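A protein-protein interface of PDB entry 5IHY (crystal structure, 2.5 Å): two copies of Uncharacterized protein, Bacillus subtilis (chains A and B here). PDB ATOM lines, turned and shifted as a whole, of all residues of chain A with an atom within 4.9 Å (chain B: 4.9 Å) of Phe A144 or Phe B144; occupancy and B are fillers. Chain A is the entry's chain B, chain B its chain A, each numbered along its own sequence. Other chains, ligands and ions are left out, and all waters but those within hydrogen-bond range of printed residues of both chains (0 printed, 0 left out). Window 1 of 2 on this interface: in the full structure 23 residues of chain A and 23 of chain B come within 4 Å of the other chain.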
ATOM      1  N   ILE A 140     -10.297 -12.736  -8.615  1.00  0.00           N
ATOM      2  CA  ILE A 140     -11.724 -12.415  -8.546  1.00  0.00           C
ATOM      3  C   ILE A 140     -12.377 -13.331  -7.510  1.00  0.00           C
ATOM      4  O   ILE A 140     -13.073 -12.863  -6.605  1.00  0.00           O
ATOM      5  CB  ILE A 140     -12.421 -12.566  -9.939  1.00  0.00           C
ATOM      6  CG1 ILE A 140     -11.939 -11.486 -10.913  1.00  0.00           C
ATOM      7  CG2 ILE A 140     -13.950 -12.493  -9.813  1.00  0.00           C
ATOM      8  CD1 ILE A 140     -12.206 -11.824 -12.367  1.00  0.00           C
ATOM      9  N   ALA A 141     -12.111 -14.629  -7.626  1.00  0.00           N
ATOM     10  CA  ALA A 141     -12.656 -15.617  -6.694  1.00  0.00           C
ATOM     11  C   ALA A 141     -12.275 -15.326  -5.240  1.00  0.00           C
ATOM     12  O   ALA A 141     -13.128 -15.366  -4.356  1.00  0.00           O
ATOM     13  CB  ALA A 141     -12.224 -17.031  -7.095  1.00  0.00           C
ATOM     14  N   ARG A 142     -10.998 -15.026  -4.998  1.00  0.00           N
ATOM     15  CA  ARG A 142     -10.502 -14.855  -3.627  1.00  0.00           C
ATOM     16  C   ARG A 142     -11.058 -13.584  -2.973  1.00  0.00           C
ATOM     17  O   ARG A 142     -11.454 -13.601  -1.802  1.00  0.00           O
ATOM     18  CB  ARG A 142      -8.968 -14.872  -3.587  1.00  0.00           C
ATOM     19  CG  ARG A 142      -8.343 -16.203  -4.008  1.00  0.00           C
ATOM     20  CD  ARG A 142      -6.822 -16.124  -4.055  1.00  0.00           C
ATOM     21  NE  ARG A 142      -6.234 -16.041  -2.709  1.00  0.00           N
ATOM     22  CZ  ARG A 142      -5.313 -15.157  -2.329  1.00  0.00           C
ATOM     23  NH1 ARG A 142      -4.832 -14.266  -3.190  1.00  0.00           N
ATOM     24  NH2 ARG A 142      -4.858 -15.177  -1.084  1.00  0.00           N
ATOM     25  N   ALA A 143     -11.117 -12.504  -3.754  1.00  0.00           N
ATOM     26  CA  ALA A 143     -11.668 -11.232  -3.306  1.00  0.00           C
ATOM     27  C   ALA A 143     -13.123 -11.330  -2.850  1.00  0.00           C
ATOM     28  O   ALA A 143     -13.502 -10.689  -1.876  1.00  0.00           O
ATOM     29  CB  ALA A 143     -11.519 -10.175  -4.393  1.00  0.00           C
ATOM     30  N   PHE A 144     -13.931 -12.128  -3.552  1.00  0.00           N
ATOM     31  CA  PHE A 144     -15.343 -12.319  -3.183  1.00  0.00           C
ATOM     32  C   PHE A 144     -15.528 -13.279  -1.996  1.00  0.00           C
ATOM     33  O   PHE A 144     -16.440 -13.098  -1.180  1.00  0.00           O
ATOM     34  CB  PHE A 144     -16.172 -12.782  -4.381  1.00  0.00           C
ATOM     35  CG  PHE A 144     -16.467 -11.698  -5.382  1.00  0.00           C
ATOM     36  CD1 PHE A 144     -17.287 -10.627  -5.048  1.00  0.00           C
ATOM     37  CD2 PHE A 144     -15.959 -11.772  -6.678  1.00  0.00           C
ATOM     38  CE1 PHE A 144     -17.572  -9.628  -5.980  1.00  0.00           C
ATOM     39  CE2 PHE A 144     -16.237 -10.777  -7.619  1.00  0.00           C
ATOM     40  CZ  PHE A 144     -17.045  -9.701  -7.265  1.00  0.00           C
ATOM     41  N   MET A 145     -14.671 -14.295  -1.909  1.00  0.00           N
ATOM     42  CA  MET A 145     -14.657 -15.185  -0.749  1.00  0.00           C
ATOM     43  C   MET A 145     -14.310 -14.420   0.525  1.00  0.00           C
ATOM     44  O   MET A 145     -14.934 -14.626   1.565  1.00  0.00           O
ATOM     45  CB  MET A 145     -13.669 -16.330  -0.947  1.00  0.00           C
ATOM     46  CG  MET A 145     -14.159 -17.391  -1.895  1.00  0.00           C
ATOM     47  SD  MET A 145     -12.894 -18.851  -2.043  1.00  0.00           S
ATOM     48  CE  MET A 145     -13.198 -19.718  -0.340  1.00  0.00           C
ATOM     49  N   PHE A 146     -13.314 -13.540   0.428  1.00  0.00           N
ATOM     50  CA  PHE A 146     -12.889 -12.706   1.544  1.00  0.00           C
ATOM     51  C   PHE A 146     -14.037 -11.809   2.032  1.00  0.00           C
ATOM     52  O   PHE A 146     -14.304 -11.727   3.239  1.00  0.00           O
ATOM     53  CB  PHE A 146     -11.665 -11.879   1.137  1.00  0.00           C
ATOM     54  CG  PHE A 146     -11.045 -11.102   2.271  1.00  0.00           C
ATOM     55  CD1 PHE A 146     -10.086 -11.693   3.095  1.00  0.00           C
ATOM     56  CD2 PHE A 146     -11.410  -9.776   2.509  1.00  0.00           C
ATOM     57  CE1 PHE A 146      -9.507 -10.982   4.142  1.00  0.00           C
ATOM     58  CE2 PHE A 146     -10.839  -9.055   3.555  1.00  0.00           C
ATOM     59  CZ  PHE A 146      -9.885  -9.659   4.374  1.00  0.00           C
ATOM     60  N   ALA A 147     -14.718 -11.158   1.088  1.00  0.00           N
ATOM     61  CA  ALA A 147     -15.869 -10.306   1.392  1.00  0.00           C
ATOM     62  C   ALA A 147     -16.960 -11.091   2.113  1.00  0.00           C
ATOM     63  O   ALA A 147     -17.557 -10.603   3.079  1.00  0.00           O
ATOM     64  CB  ALA A 147     -16.412  -9.676   0.121  1.00  0.00           C
ATOM     65  N   GLY A 148     -17.204 -12.313   1.647  1.00  0.00           N
ATOM     66  CA  GLY A 148     -18.168 -13.209   2.275  1.00  0.00           C
ATOM     67  C   GLY A 148     -17.763 -13.637   3.676  1.00  0.00           C
ATOM     68  O   GLY A 148     -18.615 -13.784   4.549  1.00  0.00           O
ATOM     69  N   LEU A 154     -21.066  -6.975  -2.028  1.00  0.00           N
ATOM     70  CA  LEU A 154     -20.588  -7.176  -3.391  1.00  0.00           C
ATOM     71  C   LEU A 154     -20.127  -5.828  -3.951  1.00  0.00           C
ATOM     72  O   LEU A 154     -19.021  -5.714  -4.456  1.00  0.00           O
ATOM     73  CB  LEU A 154     -21.684  -7.789  -4.270  1.00  0.00           C
ATOM     74  CG  LEU A 154     -21.330  -8.639  -5.499  1.00  0.00           C
ATOM     75  CD1 LEU A 154     -22.566  -9.386  -5.965  1.00  0.00           C
ATOM     76  CD2 LEU A 154     -20.753  -7.827  -6.650  1.00  0.00           C
ATOM     77  N   ALA A 161     -16.178  -5.802  -2.310  1.00  0.00           N
ATOM     78  CA  ALA A 161     -15.236  -6.442  -3.234  1.00  0.00           C
ATOM     79  C   ALA A 161     -15.071  -5.652  -4.528  1.00  0.00           C
ATOM     80  O   ALA A 161     -13.984  -5.616  -5.100  1.00  0.00           O
ATOM     81  CB  ALA A 161     -15.660  -7.870  -3.535  1.00  0.00           C
ATOM     82  N   PHE A 165     -11.401  -3.875  -6.288  1.00  0.00           N
ATOM     83  CA  PHE A 165     -10.827  -3.995  -7.639  1.00  0.00           C
ATOM     84  C   PHE A 165     -10.068  -2.738  -8.061  1.00  0.00           C
ATOM     85  O   PHE A 165      -8.936  -2.814  -8.520  1.00  0.00           O
ATOM     86  CB  PHE A 165     -11.905  -4.307  -8.695  1.00  0.00           C
ATOM     87  CG  PHE A 165     -12.512  -5.671  -8.566  1.00  0.00           C
ATOM     88  CD1 PHE A 165     -11.708  -6.802  -8.437  1.00  0.00           C
ATOM     89  CD2 PHE A 165     -13.890  -5.831  -8.589  1.00  0.00           C
ATOM     90  CE1 PHE A 165     -12.268  -8.073  -8.314  1.00  0.00           C
ATOM     91  CE2 PHE A 165     -14.464  -7.099  -8.473  1.00  0.00           C
ATOM     92  CZ  PHE A 165     -13.651  -8.223  -8.338  1.00  0.00           C
ATOM     93  N   TYR A 195     -14.396  -9.159 -16.966  1.00  0.00           N
ATOM     94  CA  TYR A 195     -15.301  -9.507 -15.873  1.00  0.00           C
ATOM     95  C   TYR A 195     -16.039  -8.276 -15.347  1.00  0.00           C
ATOM     96  O   TYR A 195     -17.254  -8.304 -15.213  1.00  0.00           O
ATOM     97  CB  TYR A 195     -14.585 -10.245 -14.725  1.00  0.00           C
ATOM     98  CG  TYR A 195     -15.518 -10.548 -13.576  1.00  0.00           C
ATOM     99  CD1 TYR A 195     -15.682  -9.643 -12.520  1.00  0.00           C
ATOM    100  CD2 TYR A 195     -16.263 -11.730 -13.553  1.00  0.00           C
ATOM    101  CE1 TYR A 195     -16.561  -9.914 -11.464  1.00  0.00           C
ATOM    102  CE2 TYR A 195     -17.147 -12.009 -12.501  1.00  0.00           C
ATOM    103  CZ  TYR A 195     -17.294 -11.097 -11.466  1.00  0.00           C
ATOM    104  OH  TYR A 195     -18.167 -11.370 -10.430  1.00  0.00           O
ATOM    105  N   LEU A 199     -20.050  -7.604 -15.387  1.00  0.00           N
ATOM    106  CA  LEU A 199     -20.726  -7.285 -14.133  1.00  0.00           C
ATOM    107  C   LEU A 199     -21.561  -6.006 -14.250  1.00  0.00           C
ATOM    108  O   LEU A 199     -22.667  -5.930 -13.721  1.00  0.00           O
ATOM    109  CB  LEU A 199     -19.702  -7.173 -12.997  1.00  0.00           C
ATOM    110  CG  LEU A 199     -20.168  -7.233 -11.536  1.00  0.00           C
ATOM    111  CD1 LEU A 199     -20.870  -8.546 -11.195  1.00  0.00           C
ATOM    112  CD2 LEU A 199     -18.985  -7.002 -10.592  1.00  0.00           C
ATOM    113  N   ILE B 140     -21.241 -15.667 -10.405  1.00  0.00           N
ATOM    114  CA  ILE B 140     -19.886 -16.030  -9.992  1.00  0.00           C
ATOM    115  C   ILE B 140     -19.556 -15.330  -8.661  1.00  0.00           C
ATOM    116  O   ILE B 140     -19.101 -15.972  -7.710  1.00  0.00           O
ATOM    117  CB  ILE B 140     -18.837 -15.672 -11.090  1.00  0.00           C
ATOM    118  CG1 ILE B 140     -18.952 -16.625 -12.282  1.00  0.00           C
ATOM    119  CG2 ILE B 140     -17.406 -15.718 -10.532  1.00  0.00           C
ATOM    120  CD1 ILE B 140     -18.618 -15.965 -13.623  1.00  0.00           C
ATOM    121  N   ALA B 141     -19.804 -14.023  -8.594  1.00  0.00           N
ATOM    122  CA  ALA B 141     -19.551 -13.253  -7.367  1.00  0.00           C
ATOM    123  C   ALA B 141     -20.267 -13.867  -6.164  1.00  0.00           C
ATOM    124  O   ALA B 141     -19.643 -14.157  -5.143  1.00  0.00           O
ATOM    125  CB  ALA B 141     -19.967 -11.796  -7.552  1.00  0.00           C
ATOM    126  N   ARG B 142     -21.571 -14.089  -6.318  1.00  0.00           N
ATOM    127  CA  ARG B 142     -22.435 -14.584  -5.244  1.00  0.00           C
ATOM    128  C   ARG B 142     -22.055 -15.971  -4.721  1.00  0.00           C
ATOM    129  O   ARG B 142     -22.159 -16.225  -3.517  1.00  0.00           O
ATOM    130  CB  ARG B 142     -23.910 -14.571  -5.679  1.00  0.00           C
ATOM    131  CG  ARG B 142     -24.555 -13.181  -5.696  1.00  0.00           C
ATOM    132  CD  ARG B 142     -26.009 -13.268  -6.148  1.00  0.00           C
ATOM    133  NE  ARG B 142     -26.885 -13.787  -5.092  1.00  0.00           N
ATOM    134  CZ  ARG B 142     -27.920 -14.605  -5.297  1.00  0.00           C
ATOM    135  NH1 ARG B 142     -28.215 -15.035  -6.521  1.00  0.00           N
ATOM    136  NH2 ARG B 142     -28.652 -15.012  -4.269  1.00  0.00           N
ATOM    137  N   ALA B 143     -21.637 -16.862  -5.622  1.00  0.00           N
ATOM    138  CA  ALA B 143     -21.201 -18.206  -5.232  1.00  0.00           C
ATOM    139  C   ALA B 143     -19.930 -18.191  -4.376  1.00  0.00           C
ATOM    140  O   ALA B 143     -19.786 -19.013  -3.460  1.00  0.00           O
ATOM    141  CB  ALA B 143     -21.002 -19.099  -6.461  1.00  0.00           C
ATOM    142  N   PHE B 144     -19.003 -17.281  -4.681  1.00  0.00           N
ATOM    143  CA  PHE B 144     -17.750 -17.212  -3.924  1.00  0.00           C
ATOM    144  C   PHE B 144     -17.945 -16.535  -2.569  1.00  0.00           C
ATOM    145  O   PHE B 144     -17.322 -16.920  -1.585  1.00  0.00           O
ATOM    146  CB  PHE B 144     -16.624 -16.565  -4.744  1.00  0.00           C
ATOM    147  CG  PHE B 144     -16.056 -17.471  -5.817  1.00  0.00           C
ATOM    148  CD1 PHE B 144     -15.337 -18.615  -5.476  1.00  0.00           C
ATOM    149  CD2 PHE B 144     -16.238 -17.182  -7.165  1.00  0.00           C
ATOM    150  CE1 PHE B 144     -14.814 -19.450  -6.455  1.00  0.00           C
ATOM    151  CE2 PHE B 144     -15.717 -18.016  -8.159  1.00  0.00           C
ATOM    152  CZ  PHE B 144     -15.006 -19.153  -7.800  1.00  0.00           C
ATOM    153  N   MET B 145     -18.829 -15.545  -2.517  1.00  0.00           N
ATOM    154  CA  MET B 145     -19.193 -14.901  -1.252  1.00  0.00           C
ATOM    155  C   MET B 145     -19.791 -15.915  -0.281  1.00  0.00           C
ATOM    156  O   MET B 145     -19.392 -15.982   0.884  1.00  0.00           O
ATOM    157  CB  MET B 145     -20.168 -13.737  -1.484  1.00  0.00           C
ATOM    158  CG  MET B 145     -19.585 -12.627  -2.352  1.00  0.00           C
ATOM    159  SD  MET B 145     -20.622 -10.983  -2.364  1.00  0.00           S
ATOM    160  CE  MET B 145     -20.514 -10.538  -0.476  1.00  0.00           C
ATOM    161  N   PHE B 146     -20.732 -16.713  -0.782  1.00  0.00           N
ATOM    162  CA  PHE B 146     -21.353 -17.777   0.000  1.00  0.00           C
ATOM    163  C   PHE B 146     -20.317 -18.775   0.541  1.00  0.00           C
ATOM    164  O   PHE B 146     -20.388 -19.174   1.706  1.00  0.00           O
ATOM    165  CB  PHE B 146     -22.417 -18.487  -0.843  1.00  0.00           C
ATOM    166  CG  PHE B 146     -23.186 -19.558  -0.099  1.00  0.00           C
ATOM    167  CD1 PHE B 146     -24.261 -19.218   0.726  1.00  0.00           C
ATOM    168  CD2 PHE B 146     -22.848 -20.906  -0.243  1.00  0.00           C
ATOM    169  CE1 PHE B 146     -24.984 -20.210   1.406  1.00  0.00           C
ATOM    170  CE2 PHE B 146     -23.558 -21.899   0.430  1.00  0.00           C
ATOM    171  CZ  PHE B 146     -24.633 -21.550   1.256  1.00  0.00           C
ATOM    172  N   ALA B 147     -19.358 -19.162  -0.303  1.00  0.00           N
ATOM    173  CA  ALA B 147     -18.285 -20.089   0.089  1.00  0.00           C
ATOM    174  C   ALA B 147     -17.447 -19.548   1.248  1.00  0.00           C
ATOM    175  O   ALA B 147     -17.140 -20.273   2.197  1.00  0.00           O
ATOM    176  CB  ALA B 147     -17.396 -20.419  -1.106  1.00  0.00           C
ATOM    177  N   GLY B 148     -17.093 -18.268   1.168  1.00  0.00           N
ATOM    178  CA  GLY B 148     -16.342 -17.607   2.233  1.00  0.00           C
ATOM    179  C   GLY B 148     -17.137 -17.503   3.519  1.00  0.00           C
ATOM    180  O   GLY B 148     -16.575 -17.611   4.609  1.00  0.00           O
ATOM    181  N   LEU B 154     -12.245 -22.837  -2.322  1.00  0.00           N
ATOM    182  CA  LEU B 154     -12.418 -22.382  -3.701  1.00  0.00           C
ATOM    183  C   LEU B 154     -12.695 -23.609  -4.569  1.00  0.00           C
ATOM    184  O   LEU B 154     -13.570 -23.579  -5.438  1.00  0.00           O
ATOM    185  CB  LEU B 154     -11.163 -21.638  -4.188  1.00  0.00           C
ATOM    186  CG  LEU B 154     -11.228 -20.533  -5.262  1.00  0.00           C
ATOM    187  CD1 LEU B 154      -9.920 -19.736  -5.279  1.00  0.00           C
ATOM    188  CD2 LEU B 154     -11.529 -21.074  -6.661  1.00  0.00           C
ATOM    189  N   ALA B 161     -16.874 -23.911  -3.895  1.00  0.00           N
ATOM    190  CA  ALA B 161     -17.505 -23.064  -4.909  1.00  0.00           C
ATOM    191  C   ALA B 161     -17.414 -23.659  -6.313  1.00  0.00           C
ATOM    192  O   ALA B 161     -18.377 -23.599  -7.074  1.00  0.00           O
ATOM    193  CB  ALA B 161     -16.908 -21.686  -4.880  1.00  0.00           C
ATOM    194  N   PHE B 165     -20.541 -24.978  -9.154  1.00  0.00           N
ATOM    195  CA  PHE B 165     -20.729 -24.635 -10.561  1.00  0.00           C
ATOM    196  C   PHE B 165     -21.209 -25.845 -11.355  1.00  0.00           C
ATOM    197  O   PHE B 165     -22.226 -25.774 -12.050  1.00  0.00           O
ATOM    198  CB  PHE B 165     -19.438 -24.094 -11.184  1.00  0.00           C
ATOM    199  CG  PHE B 165     -19.164 -22.655 -10.867  1.00  0.00           C
ATOM    200  CD1 PHE B 165     -19.688 -21.641 -11.660  1.00  0.00           C
ATOM    201  CD2 PHE B 165     -18.367 -22.312  -9.782  1.00  0.00           C
ATOM    202  CE1 PHE B 165     -19.436 -20.303 -11.358  1.00  0.00           C
ATOM    203  CE2 PHE B 165     -18.103 -20.978  -9.471  1.00  0.00           C
ATOM    204  CZ  PHE B 165     -18.632 -19.973 -10.258  1.00  0.00           C
ATOM    205  N   TYR B 195     -15.396 -18.261 -17.689  1.00  0.00           N
ATOM    206  CA  TYR B 195     -14.781 -18.094 -16.390  1.00  0.00           C
ATOM    207  C   TYR B 195     -14.173 -19.413 -15.890  1.00  0.00           C
ATOM    208  O   TYR B 195     -13.049 -19.418 -15.375  1.00  0.00           O
ATOM    209  CB  TYR B 195     -15.772 -17.519 -15.374  1.00  0.00           C
ATOM    210  CG  TYR B 195     -15.144 -17.342 -14.016  1.00  0.00           C
ATOM    211  CD1 TYR B 195     -15.128 -18.387 -13.100  1.00  0.00           C
ATOM    212  CD2 TYR B 195     -14.527 -16.143 -13.661  1.00  0.00           C
ATOM    213  CE1 TYR B 195     -14.532 -18.246 -11.863  1.00  0.00           C
ATOM    214  CE2 TYR B 195     -13.924 -15.987 -12.416  1.00  0.00           C
ATOM    215  CZ  TYR B 195     -13.928 -17.049 -11.527  1.00  0.00           C
ATOM    216  OH  TYR B 195     -13.334 -16.922 -10.296  1.00  0.00           O
ATOM    217  N   LEU B 199     -10.199 -20.339 -15.137  1.00  0.00           N
ATOM    218  CA  LEU B 199      -9.699 -20.968 -13.922  1.00  0.00           C
ATOM    219  C   LEU B 199      -8.888 -22.224 -14.217  1.00  0.00           C
ATOM    220  O   LEU B 199      -7.846 -22.453 -13.600  1.00  0.00           O
ATOM    221  CB  LEU B 199     -10.839 -21.296 -12.949  1.00  0.00           C
ATOM    222  CG  LEU B 199     -11.333 -20.206 -11.995  1.00  0.00           C
ATOM    223  CD1 LEU B 199     -12.481 -20.744 -11.172  1.00  0.00           C
ATOM    224  CD2 LEU B 199     -10.229 -19.696 -11.079  1.00  0.00           C
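Ala A141 touches Leu B154, and with the chains exchanged Leu A154 touches Ala B141.
Ala A141 touches Tyr B195, and with the chains exchanged Tyr A195 touches Ala B141.
Phe A144 touches Met B145, and with the chains exchanged Met A145 touches Phe B144.
Met A145 touches Leu B154, and with the chains exchanged Leu A154 touches Met B145.
Positions printed for both chains: 140, 141, 142, 143, 144, 145, 146, 147, 148, 154, 161, 165, 195 and 199.
Of the 14 pairs that touch across the chains among the printed residues, 14 have their exchanged pair printed and touching as well.
Of the 14 printed residues of chain B, 6 touch a printed residue of chain A.
Printed residues of chain A that touch a printed residue of chain B: Ala A141, Phe A144, Met A145, Gly A148, Leu A154 and Tyr A195.
Hydrophobic or aromatic side chains of chain A that line the printed part of chain B: Ala A141, Phe A144, Met A145, Leu A154 and Tyr A195.
Among the printed residues, 14 pairs touch across the chains.
Among the printed residues, no Asp or Glu carboxylate lies within 4 Å of a Lys or Arg side-chain nitrogen of the other chain.
Phe A146 touches none of the printed residues of chain B.
Printed residues of chain B within 4 Å of Leu A154: Ala B141 (3.9 Å) and Met B145 (3.9 Å).
Of the printed residues of chain A, Ala B141 touches Phe A144 (3.6 Å), Leu A154 (3.9 Å) and Tyr A195 (3.4 Å).
Ala B143 touches none of the printed residues of chain A.
Phe B144 touches three residues of chain A.
The nearest printed residue of chain B that does not touch Phe A144 is Ile B140 (5.3 Å).
Among the printed residues, merely in contact across the chains: Ala A141 with Phe B144 (3.6 Å), Ala A141 with Leu B154 (3.99 Å), Ala A141 with Tyr B195 (3.4 Å), Phe A144 with Ala B141 (3.6 Å), Phe A144 with Phe B144 (3.8 Å), Phe A144 with Met B145 (3.3 Å), Met A145 with Phe B144 (3.2 Å), Met A145 with Gly B148 (3.4 Å), Met A145 with Leu B154 (3.8 Å), Gly A148 with Met B145 (3.3 Å), Gly A148 with Gly B148 (3.9 Å), Leu A154 with Ala B141 (3.9 Å), Leu A154 with Met B145 (3.9 Å) and Tyr A195 with Ala B141 (3.4 Å).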
